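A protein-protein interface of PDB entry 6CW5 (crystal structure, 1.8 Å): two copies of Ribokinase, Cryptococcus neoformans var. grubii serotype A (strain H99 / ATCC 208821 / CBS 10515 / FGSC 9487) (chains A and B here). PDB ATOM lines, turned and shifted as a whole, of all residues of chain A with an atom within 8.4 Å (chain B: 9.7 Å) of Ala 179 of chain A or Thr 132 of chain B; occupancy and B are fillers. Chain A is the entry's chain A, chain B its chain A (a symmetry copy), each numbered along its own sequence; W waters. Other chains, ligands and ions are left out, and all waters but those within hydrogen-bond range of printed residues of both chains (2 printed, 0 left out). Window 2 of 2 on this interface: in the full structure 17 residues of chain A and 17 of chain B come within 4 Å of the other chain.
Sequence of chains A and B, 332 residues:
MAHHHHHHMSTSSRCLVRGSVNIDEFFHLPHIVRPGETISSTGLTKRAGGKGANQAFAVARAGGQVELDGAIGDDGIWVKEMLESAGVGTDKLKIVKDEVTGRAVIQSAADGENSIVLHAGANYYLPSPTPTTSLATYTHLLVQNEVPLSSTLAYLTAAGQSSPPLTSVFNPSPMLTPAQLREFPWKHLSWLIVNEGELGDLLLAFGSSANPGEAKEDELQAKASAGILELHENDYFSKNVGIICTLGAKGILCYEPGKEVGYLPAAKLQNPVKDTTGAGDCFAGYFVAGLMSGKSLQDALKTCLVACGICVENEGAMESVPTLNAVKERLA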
ATOM      1  N   LEU A 149      -7.958 -20.119 -19.461  1.00  0.00           N
ATOM      2  CA  LEU A 149      -7.532 -20.981 -18.356  1.00  0.00           C
ATOM      3  C   LEU A 149      -6.600 -20.239 -17.409  1.00  0.00           C
ATOM      4  O   LEU A 149      -6.632 -20.464 -16.196  1.00  0.00           O
ATOM      5  CB  LEU A 149      -6.846 -22.237 -18.886  1.00  0.00           C
ATOM      6  CG  LEU A 149      -6.327 -23.235 -17.818  1.00  0.00           C
ATOM      7  CD1 LEU A 149      -7.465 -23.704 -16.907  1.00  0.00           C
ATOM      8  CD2 LEU A 149      -5.617 -24.444 -18.532  1.00  0.00           C
ATOM      9  N   LEU A 176     -10.404 -29.773 -20.165  1.00  0.00           N
ATOM     10  CA  LEU A 176      -9.043 -29.294 -20.357  1.00  0.00           C
ATOM     11  C   LEU A 176      -8.255 -30.327 -21.157  1.00  0.00           C
ATOM     12  O   LEU A 176      -8.630 -31.503 -21.210  1.00  0.00           O
ATOM     13  CB  LEU A 176      -8.360 -29.054 -18.987  1.00  0.00           C
ATOM     14  CG  LEU A 176      -8.834 -27.804 -18.206  1.00  0.00           C
ATOM     15  CD1 LEU A 176     -10.282 -27.947 -17.744  1.00  0.00           C
ATOM     16  CD2 LEU A 176      -7.932 -27.585 -16.976  1.00  0.00           C
ATOM     17  N   THR A 177      -7.149 -29.889 -21.787  1.00  0.00           N
ATOM     18  CA  THR A 177      -6.284 -30.843 -22.470  1.00  0.00           C
ATOM     19  C   THR A 177      -5.605 -31.734 -21.433  1.00  0.00           C
ATOM     20  O   THR A 177      -5.484 -31.360 -20.259  1.00  0.00           O
ATOM     21  CB  THR A 177      -5.224 -30.148 -23.336  1.00  0.00           C
ATOM     22  OG1 THR A 177      -4.211 -29.562 -22.496  1.00  0.00           O
ATOM     23  CG2 THR A 177      -5.840 -29.046 -24.189  1.00  0.00           C
ATOM     24  N   PRO A 178      -5.145 -32.925 -21.834  1.00  0.00           N
ATOM     25  CA  PRO A 178      -4.509 -33.801 -20.830  1.00  0.00           C
ATOM     26  C   PRO A 178      -3.313 -33.144 -20.175  1.00  0.00           C
ATOM     27  O   PRO A 178      -3.136 -33.252 -18.957  1.00  0.00           O
ATOM     28  CB  PRO A 178      -4.137 -35.052 -21.651  1.00  0.00           C
ATOM     29  CG  PRO A 178      -5.247 -35.103 -22.700  1.00  0.00           C
ATOM     30  CD  PRO A 178      -5.471 -33.638 -23.075  1.00  0.00           C
ATOM     31  N   ALA A 179      -2.503 -32.406 -20.937  1.00  0.00           N
ATOM     32  CA  ALA A 179      -1.362 -31.745 -20.305  1.00  0.00           C
ATOM     33  C   ALA A 179      -1.822 -30.683 -19.304  1.00  0.00           C
ATOM     34  O   ALA A 179      -1.248 -30.539 -18.217  1.00  0.00           O
ATOM     35  CB  ALA A 179      -0.453 -31.137 -21.381  1.00  0.00           C
ATOM     36  N   GLN A 180      -2.860 -29.930 -19.651  1.00  0.00           N
ATOM     37  CA  GLN A 180      -3.383 -28.954 -18.702  1.00  0.00           C
ATOM     38  C   GLN A 180      -3.873 -29.626 -17.426  1.00  0.00           C
ATOM     39  O   GLN A 180      -3.657 -29.111 -16.330  1.00  0.00           O
ATOM     40  CB  GLN A 180      -4.517 -28.166 -19.348  1.00  0.00           C
ATOM     41  CG  GLN A 180      -4.014 -27.190 -20.396  1.00  0.00           C
ATOM     42  CD  GLN A 180      -5.130 -26.620 -21.246  1.00  0.00           C
ATOM     43  OE1 GLN A 180      -6.288 -27.078 -21.201  1.00  0.00           O
ATOM     44  NE2 GLN A 180      -4.793 -25.591 -22.020  1.00  0.00           N
ATOM     45  N   LEU A 181      -4.570 -30.760 -17.549  1.00  0.00           N
ATOM     46  CA  LEU A 181      -5.013 -31.478 -16.355  1.00  0.00           C
ATOM     47  C   LEU A 181      -3.820 -31.914 -15.511  1.00  0.00           C
ATOM     48  O   LEU A 181      -3.826 -31.763 -14.280  1.00  0.00           O
ATOM     49  CB  LEU A 181      -5.867 -32.700 -16.751  1.00  0.00           C
ATOM     50  CG  LEU A 181      -7.187 -32.347 -17.451  1.00  0.00           C
ATOM     51  CD1 LEU A 181      -7.758 -33.656 -18.046  1.00  0.00           C
ATOM     52  CD2 LEU A 181      -8.159 -31.740 -16.428  1.00  0.00           C
ATOM     53  N   ARG A 182      -2.771 -32.429 -16.153  1.00  0.00           N
ATOM     54  CA  ARG A 182      -1.619 -32.897 -15.387  1.00  0.00           C
ATOM     55  C   ARG A 182      -0.866 -31.777 -14.696  1.00  0.00           C
ATOM     56  O   ARG A 182      -0.176 -32.034 -13.695  1.00  0.00           O
ATOM     57  CB  ARG A 182      -0.645 -33.663 -16.288  1.00  0.00           C
ATOM     58  CG  ARG A 182      -1.198 -34.977 -16.779  1.00  0.00           C
ATOM     59  CD  ARG A 182      -0.142 -35.753 -17.584  1.00  0.00           C
ATOM     60  NE  ARG A 182       0.123 -35.187 -18.908  1.00  0.00           N
ATOM     61  CZ  ARG A 182      -0.468 -35.608 -20.023  1.00  0.00           C
ATOM     62  NH1 ARG A 182      -1.390 -36.573 -19.979  1.00  0.00           N
ATOM     63  NH2 ARG A 182      -0.152 -35.056 -21.181  1.00  0.00           N
ATOM     64  N   GLU A 183      -1.002 -30.544 -15.172  1.00  0.00           N
ATOM     65  CA  GLU A 183      -0.261 -29.422 -14.594  1.00  0.00           C
ATOM     66  C   GLU A 183      -1.131 -28.547 -13.710  1.00  0.00           C
ATOM     67  O   GLU A 183      -0.634 -27.566 -13.149  1.00  0.00           O
ATOM     68  CB  GLU A 183       0.343 -28.575 -15.727  1.00  0.00           C
ATOM     69  CG  GLU A 183       1.485 -29.328 -16.433  1.00  0.00           C
ATOM     70  CD  GLU A 183       1.709 -28.881 -17.861  1.00  0.00           C
ATOM     71  OE1 GLU A 183       1.462 -27.691 -18.153  1.00  0.00           O
ATOM     72  OE2 GLU A 183       2.119 -29.736 -18.686  1.00  0.00           O
ATOM     73  N   PHE A 184      -2.416 -28.867 -13.619  1.00  0.00           N
ATOM     74  CA  PHE A 184      -3.366 -28.064 -12.864  1.00  0.00           C
ATOM     75  C   PHE A 184      -3.035 -28.088 -11.372  1.00  0.00           C
ATOM     76  O   PHE A 184      -2.601 -29.121 -10.835  1.00  0.00           O
ATOM     77  CB  PHE A 184      -4.765 -28.609 -13.151  1.00  0.00           C
ATOM     78  CG  PHE A 184      -5.890 -27.696 -12.764  1.00  0.00           C
ATOM     79  CD1 PHE A 184      -6.381 -26.752 -13.668  1.00  0.00           C
ATOM     80  CD2 PHE A 184      -6.497 -27.828 -11.527  1.00  0.00           C
ATOM     81  CE1 PHE A 184      -7.438 -25.922 -13.328  1.00  0.00           C
ATOM     82  CE2 PHE A 184      -7.583 -27.009 -11.174  1.00  0.00           C
ATOM     83  CZ  PHE A 184      -8.041 -26.054 -12.074  1.00  0.00           C
ATOM     84  N   TRP A 186      -4.057 -28.787  -8.443  1.00  0.00           N
ATOM     85  CA  TRP A 186      -5.080 -29.477  -7.663  1.00  0.00           C
ATOM     86  C   TRP A 186      -4.944 -29.222  -6.172  1.00  0.00           C
ATOM     87  O   TRP A 186      -5.943 -29.292  -5.448  1.00  0.00           O
ATOM     88  CB  TRP A 186      -4.998 -30.981  -7.923  1.00  0.00           C
ATOM     89  CG  TRP A 186      -5.241 -31.267  -9.385  1.00  0.00           C
ATOM     90  CD1 TRP A 186      -4.314 -31.686 -10.295  1.00  0.00           C
ATOM     91  CD2 TRP A 186      -6.476 -31.120 -10.099  1.00  0.00           C
ATOM     92  NE1 TRP A 186      -4.900 -31.818 -11.531  1.00  0.00           N
ATOM     93  CE2 TRP A 186      -6.226 -31.486 -11.441  1.00  0.00           C
ATOM     94  CE3 TRP A 186      -7.774 -30.729  -9.737  1.00  0.00           C
ATOM     95  CZ2 TRP A 186      -7.227 -31.468 -12.435  1.00  0.00           C
ATOM     96  CZ3 TRP A 186      -8.769 -30.720 -10.719  1.00  0.00           C
ATOM     97  CH2 TRP A 186      -8.484 -31.081 -12.056  1.00  0.00           C
ATOM     98  N   ALA A 205      -6.014 -38.929 -18.534  1.00  0.00           N
ATOM     99  CA  ALA A 205      -4.896 -37.997 -18.633  1.00  0.00           C
ATOM    100  C   ALA A 205      -3.829 -38.320 -17.599  1.00  0.00           C
ATOM    101  O   ALA A 205      -2.658 -37.959 -17.788  1.00  0.00           O
ATOM    102  CB  ALA A 205      -5.396 -36.550 -18.469  1.00  0.00           C
ATOM    103  N   PHE A 206      -4.208 -38.968 -16.502  1.00  0.00           N
ATOM    104  CA  PHE A 206      -3.292 -39.248 -15.407  1.00  0.00           C
ATOM    105  C   PHE A 206      -2.695 -40.649 -15.511  1.00  0.00           C
ATOM    106  O   PHE A 206      -2.144 -41.166 -14.526  1.00  0.00           O
ATOM    107  CB  PHE A 206      -4.008 -39.069 -14.053  1.00  0.00           C
ATOM    108  CG  PHE A 206      -4.444 -37.639 -13.792  1.00  0.00           C
ATOM    109  CD1 PHE A 206      -3.972 -36.614 -14.615  1.00  0.00           C
ATOM    110  CD2 PHE A 206      -5.273 -37.336 -12.711  1.00  0.00           C
ATOM    111  CE1 PHE A 206      -4.360 -35.289 -14.391  1.00  0.00           C
ATOM    112  CE2 PHE A 206      -5.656 -36.023 -12.463  1.00  0.00           C
ATOM    113  CZ  PHE A 206      -5.200 -35.008 -13.311  1.00  0.00           C
ATOM    114  N   TYR A 236      -0.638 -37.194 -10.021  1.00  0.00           N
ATOM    115  CA  TYR A 236      -0.927 -35.958 -10.747  1.00  0.00           C
ATOM    116  C   TYR A 236      -2.006 -35.137 -10.070  1.00  0.00           C
ATOM    117  O   TYR A 236      -2.142 -33.939 -10.365  1.00  0.00           O
ATOM    118  CB  TYR A 236      -1.380 -36.240 -12.189  1.00  0.00           C
ATOM    119  CG  TYR A 236      -0.308 -36.698 -13.149  1.00  0.00           C
ATOM    120  CD1 TYR A 236       0.687 -35.829 -13.582  1.00  0.00           C
ATOM    121  CD2 TYR A 236      -0.311 -37.998 -13.660  1.00  0.00           C
ATOM    122  CE1 TYR A 236       1.673 -36.252 -14.474  1.00  0.00           C
ATOM    123  CE2 TYR A 236       0.676 -38.429 -14.554  1.00  0.00           C
ATOM    124  CZ  TYR A 236       1.653 -37.550 -14.956  1.00  0.00           C
ATOM    125  OH  TYR A 236       2.624 -37.961 -15.833  1.00  0.00           O
ATOM    126  N   ASP B  69       6.053 -15.466 -27.969  1.00  0.00           N
ATOM    127  CA  ASP B  69       4.686 -15.968 -27.840  1.00  0.00           C
ATOM    128  C   ASP B  69       3.799 -14.765 -27.502  1.00  0.00           C
ATOM    129  O   ASP B  69       3.984 -14.127 -26.467  1.00  0.00           O
ATOM    130  CB  ASP B  69       4.634 -17.050 -26.747  1.00  0.00           C
ATOM    131  CG  ASP B  69       3.253 -17.636 -26.533  1.00  0.00           C
ATOM    132  OD1 ASP B  69       2.240 -16.987 -26.844  1.00  0.00           O
ATOM    133  OD2 ASP B  69       3.183 -18.735 -25.979  1.00  0.00           O
ATOM    134  N   LYS B  92       4.471 -18.854 -32.552  1.00  0.00           N
ATOM    135  CA  LYS B  92       3.502 -18.570 -31.500  1.00  0.00           C
ATOM    136  C   LYS B  92       3.106 -17.106 -31.461  1.00  0.00           C
ATOM    137  O   LYS B  92       2.501 -16.670 -30.478  1.00  0.00           O
ATOM    138  CB  LYS B  92       4.059 -18.980 -30.137  1.00  0.00           C
ATOM    139  CG  LYS B  92       4.521 -20.444 -30.070  1.00  0.00           C
ATOM    140  CD  LYS B  92       3.365 -21.402 -30.065  1.00  0.00           C
ATOM    141  CE  LYS B  92       3.848 -22.821 -29.722  1.00  0.00           C
ATOM    142  NZ  LYS B  92       4.752 -23.402 -30.768  1.00  0.00           N
ATOM    143  N   LYS B  94       0.649 -14.829 -32.808  1.00  0.00           N
ATOM    144  CA  LYS B  94      -0.625 -15.008 -33.465  1.00  0.00           C
ATOM    145  C   LYS B  94      -1.038 -13.712 -34.144  1.00  0.00           C
ATOM    146  O   LYS B  94      -0.796 -12.626 -33.619  1.00  0.00           O
ATOM    147  CB  LYS B  94      -1.683 -15.438 -32.447  1.00  0.00           C
ATOM    148  CG  LYS B  94      -1.394 -16.861 -31.874  1.00  0.00           C
ATOM    149  CD  LYS B  94      -2.028 -17.114 -30.510  1.00  0.00           C
ATOM    150  CE  LYS B  94      -1.267 -16.446 -29.364  1.00  0.00           C
ATOM    151  NZ  LYS B  94       0.068 -17.047 -29.053  1.00  0.00           N
ATOM    152  N   PRO B 127      -6.365 -16.762 -27.244  1.00  0.00           N
ATOM    153  CA  PRO B 127      -7.208 -17.560 -28.140  1.00  0.00           C
ATOM    154  C   PRO B 127      -8.060 -18.554 -27.378  1.00  0.00           C
ATOM    155  O   PRO B 127      -7.655 -19.086 -26.341  1.00  0.00           O
ATOM    156  CB  PRO B 127      -6.188 -18.294 -29.025  1.00  0.00           C
ATOM    157  CG  PRO B 127      -4.969 -18.417 -28.144  1.00  0.00           C
ATOM    158  CD  PRO B 127      -4.935 -17.090 -27.379  1.00  0.00           C
ATOM    159  N   SER B 128      -9.276 -18.813 -27.933  1.00  0.00           N
ATOM    160  CA  SER B 128     -10.158 -19.848 -27.417  1.00  0.00           C
ATOM    161  C   SER B 128     -10.190 -21.032 -28.381  1.00  0.00           C
ATOM    162  O   SER B 128     -10.182 -20.825 -29.594  1.00  0.00           O
ATOM    163  CB  SER B 128     -11.580 -19.286 -27.238  1.00  0.00           C
ATOM    164  OG  SER B 128     -12.508 -20.325 -26.942  1.00  0.00           O
ATOM    165  N   PRO B 129     -10.192 -22.284 -27.890  1.00  0.00           N
ATOM    166  CA  PRO B 129      -9.983 -22.647 -26.474  1.00  0.00           C
ATOM    167  C   PRO B 129      -8.564 -22.408 -26.083  1.00  0.00           C
ATOM    168  O   PRO B 129      -7.725 -22.201 -26.960  1.00  0.00           O
ATOM    169  CB  PRO B 129     -10.295 -24.137 -26.449  1.00  0.00           C
ATOM    170  CG  PRO B 129      -9.846 -24.579 -27.777  1.00  0.00           C
ATOM    171  CD  PRO B 129     -10.273 -23.480 -28.733  1.00  0.00           C
ATOM    172  N   THR B 130      -8.295 -22.382 -24.783  1.00  0.00           N
ATOM    173  CA  THR B 130      -6.937 -22.178 -24.327  1.00  0.00           C
ATOM    174  C   THR B 130      -6.130 -23.414 -24.685  1.00  0.00           C
ATOM    175  O   THR B 130      -6.482 -24.517 -24.252  1.00  0.00           O
ATOM    176  CB  THR B 130      -6.902 -21.957 -22.824  1.00  0.00           C
ATOM    177  OG1 THR B 130      -7.700 -20.815 -22.508  1.00  0.00           O
ATOM    178  CG2 THR B 130      -5.450 -21.693 -22.372  1.00  0.00           C
ATOM    179  N   PRO B 131      -5.080 -23.300 -25.474  1.00  0.00           N
ATOM    180  CA  PRO B 131      -4.357 -24.500 -25.892  1.00  0.00           C
ATOM    181  C   PRO B 131      -3.303 -24.896 -24.860  1.00  0.00           C
ATOM    182  O   PRO B 131      -2.965 -24.132 -23.953  1.00  0.00           O
ATOM    183  CB  PRO B 131      -3.699 -24.066 -27.204  1.00  0.00           C
ATOM    184  CG  PRO B 131      -3.408 -22.608 -26.998  1.00  0.00           C
ATOM    185  CD  PRO B 131      -4.537 -22.069 -26.092  1.00  0.00           C
ATOM    186  N   THR B 132      -2.830 -26.133 -25.018  1.00  0.00           N
ATOM    187  CA  THR B 132      -1.629 -26.557 -24.308  1.00  0.00           C
ATOM    188  C   THR B 132      -0.484 -25.656 -24.738  1.00  0.00           C
ATOM    189  O   THR B 132      -0.247 -25.472 -25.938  1.00  0.00           O
ATOM    190  CB  THR B 132      -1.281 -28.002 -24.657  1.00  0.00           C
ATOM    191  OG1 THR B 132      -2.381 -28.879 -24.375  1.00  0.00           O
ATOM    192  CG2 THR B 132      -0.008 -28.490 -23.924  1.00  0.00           C
ATOM    193  N   THR B 133       0.254 -25.145 -23.772  1.00  0.00           N
ATOM    194  CA  THR B 133       1.552 -24.531 -24.044  1.00  0.00           C
ATOM    195  C   THR B 133       2.620 -25.326 -23.302  1.00  0.00           C
ATOM    196  O   THR B 133       2.545 -25.509 -22.083  1.00  0.00           O
ATOM    197  CB  THR B 133       1.569 -23.049 -23.659  1.00  0.00           C
ATOM    198  OG1 THR B 133       0.560 -22.346 -24.412  1.00  0.00           O
ATOM    199  CG2 THR B 133       2.939 -22.427 -23.971  1.00  0.00           C
ATOM    200  N   SER B 134       3.531 -25.911 -24.053  1.00  0.00           N
ATOM    201  CA  SER B 134       4.612 -26.693 -23.494  1.00  0.00           C
ATOM    202  C   SER B 134       5.828 -25.799 -23.405  1.00  0.00           C
ATOM    203  O   SER B 134       6.060 -24.954 -24.280  1.00  0.00           O
ATOM    204  CB  SER B 134       4.925 -27.907 -24.360  1.00  0.00           C
ATOM    205  OG  SER B 134       6.017 -28.656 -23.833  1.00  0.00           O
ATOM    206  N   LEU B 135       6.582 -25.968 -22.334  1.00  0.00           N
ATOM    207  CA  LEU B 135       7.865 -25.303 -22.204  1.00  0.00           C
ATOM    208  C   LEU B 135       9.008 -26.255 -22.493  1.00  0.00           C
ATOM    209  O   LEU B 135      10.163 -25.934 -22.197  1.00  0.00           O
ATOM    210  CB  LEU B 135       8.006 -24.701 -20.803  1.00  0.00           C
ATOM    211  CG  LEU B 135       6.937 -23.669 -20.475  1.00  0.00           C
ATOM    212  CD1 LEU B 135       7.231 -23.058 -19.124  1.00  0.00           C
ATOM    213  CD2 LEU B 135       6.838 -22.547 -21.540  1.00  0.00           C
ATOM    214  N   ALA B 136       8.699 -27.418 -23.086  1.00  0.00           N
ATOM    215  CA  ALA B 136       9.656 -28.515 -23.158  1.00  0.00           C
ATOM    216  C   ALA B 136      10.949 -28.115 -23.860  1.00  0.00           C
ATOM    217  O   ALA B 136      12.026 -28.596 -23.491  1.00  0.00           O
ATOM    218  CB  ALA B 136       9.021 -29.714 -23.867  1.00  0.00           C
ATOM    219  N   TYR B 155       2.720 -18.676 -17.184  1.00  0.00           N
ATOM    220  CA  TYR B 155       3.977 -19.107 -17.796  1.00  0.00           C
ATOM    221  C   TYR B 155       5.101 -19.178 -16.766  1.00  0.00           C
ATOM    222  O   TYR B 155       5.900 -20.128 -16.767  1.00  0.00           O
ATOM    223  CB  TYR B 155       4.382 -18.156 -18.917  1.00  0.00           C
ATOM    224  CG  TYR B 155       3.638 -18.383 -20.215  1.00  0.00           C
ATOM    225  CD1 TYR B 155       2.263 -18.193 -20.296  1.00  0.00           C
ATOM    226  CD2 TYR B 155       4.314 -18.806 -21.355  1.00  0.00           C
ATOM    227  CE1 TYR B 155       1.593 -18.400 -21.518  1.00  0.00           C
ATOM    228  CE2 TYR B 155       3.662 -19.003 -22.557  1.00  0.00           C
ATOM    229  CZ  TYR B 155       2.296 -18.799 -22.629  1.00  0.00           C
ATOM    230  OH  TYR B 155       1.636 -19.017 -23.832  1.00  0.00           O
ATOM    231  N   ALA B 158       4.578 -22.308 -14.695  1.00  0.00           N
ATOM    232  CA  ALA B 158       4.972 -23.490 -15.452  1.00  0.00           C
ATOM    233  C   ALA B 158       6.490 -23.602 -15.543  1.00  0.00           C
ATOM    234  O   ALA B 158       7.051 -24.716 -15.524  1.00  0.00           O
ATOM    235  CB  ALA B 158       4.359 -23.434 -16.858  1.00  0.00           C
ATOM    236  N   GLN B 161       7.832 -24.748 -12.123  1.00  0.00           N
ATOM    237  CA  GLN B 161       7.459 -26.113 -11.781  1.00  0.00           C
ATOM    238  C   GLN B 161       7.960 -27.144 -12.777  1.00  0.00           C
ATOM    239  O   GLN B 161       7.700 -28.332 -12.583  1.00  0.00           O
ATOM    240  CB  GLN B 161       5.941 -26.223 -11.645  1.00  0.00           C
ATOM    241  CG  GLN B 161       5.412 -25.343 -10.528  1.00  0.00           C
ATOM    242  CD  GLN B 161       3.922 -25.441 -10.369  1.00  0.00           C
ATOM    243  OE1 GLN B 161       3.191 -25.809 -11.305  1.00  0.00           O
ATOM    244  NE2 GLN B 161       3.450 -25.115  -9.184  1.00  0.00           N
HETATM  245  O   HOH W   1       0.238 -26.026 -11.090  1.00  0.00           O
HETATM  246  O   HOH W   2      -9.816 -22.384 -20.935  1.00  0.00           O
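Water W1 bridges O of Glu 183 of chain A and OE1 of Gln 161 of chain B.
Water W2 lies within hydrogen-bond range of OG1 of Thr 130 of chain B (3.1 Å) and N of Leu 149 of chain A (3.3 Å).
The backbone NH (N) of Thr 177 of chain A is in hydrogen-bond range of the side-chain amide oxygen (OE1) of Gln 180 of chain A (3.0 Å).
Printed residues of chain B within 4 Å of Leu 149 of chain A: Thr 130.
Thr 177 of chain A touches one residue of chain B.
No residue of chain B comes within 4 Å of Pro 178 of chain A.
Of chain B, only Thr 132 (3.7 Å) comes within 4 Å of Ala 179 of chain A.
Gln 180 of chain A touches just these residues of chain B: Thr 130 (3.0 Å), Pro 131 (3.0 Å) and Thr 132 (3.6 Å).
No residue of chain B comes within 4 Å of Arg 182 of chain A.
Of the printed residues of chain A, Thr 130 of chain B touches Leu 149 and Gln 180.
Of the printed residues of chain A, Pro 131 of chain B touches Gln 180 (3.0 Å).
Thr 132 of chain B touches just these residues of chain A: Thr 177, Ala 179 and Gln 180.
No position is printed for both chains.
Of the 6 pairs that touch across the chains among the printed residues, none has its exchanged pair printed and touching as well.
Printed residues of chain B that touch a printed residue of chain A: Thr 130, Pro 131 and Thr 132.
Along chain B the printed residues that touch a printed residue of chain A span positions 130 to 132.
Of the 14 printed residues of chain A, 4 touch a printed residue of chain B.
Among the printed residues, 6 pairs touch across the chains.
Among the printed residues, no Asp or Glu carboxylate lies within 4 Å of a Lys or Arg side-chain nitrogen of the other chain.
NE2 of Gln 180 of chain A is in hydrogen-bond range of O of Pro 131 of chain B (3.0 Å).
NE2 of Gln 180 of chain A lies within hydrogen-bond range of O of Thr 130 of chain B (3.0 Å).
N of Leu 149 of chain A is in hydrogen-bond range of OG1 of Thr 130 of chain B, at 3.1 Å.
OG1 of Thr 177 of chain A sits at hydrogen-bond distance from OG1 of Thr 132 of chain B (2.7 Å).
Ala 179 of chain A touches Thr 132 of chain B.
NE2 of Gln 180 of chain A touches N of Thr 132 of chain B, 3.6 Å away.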
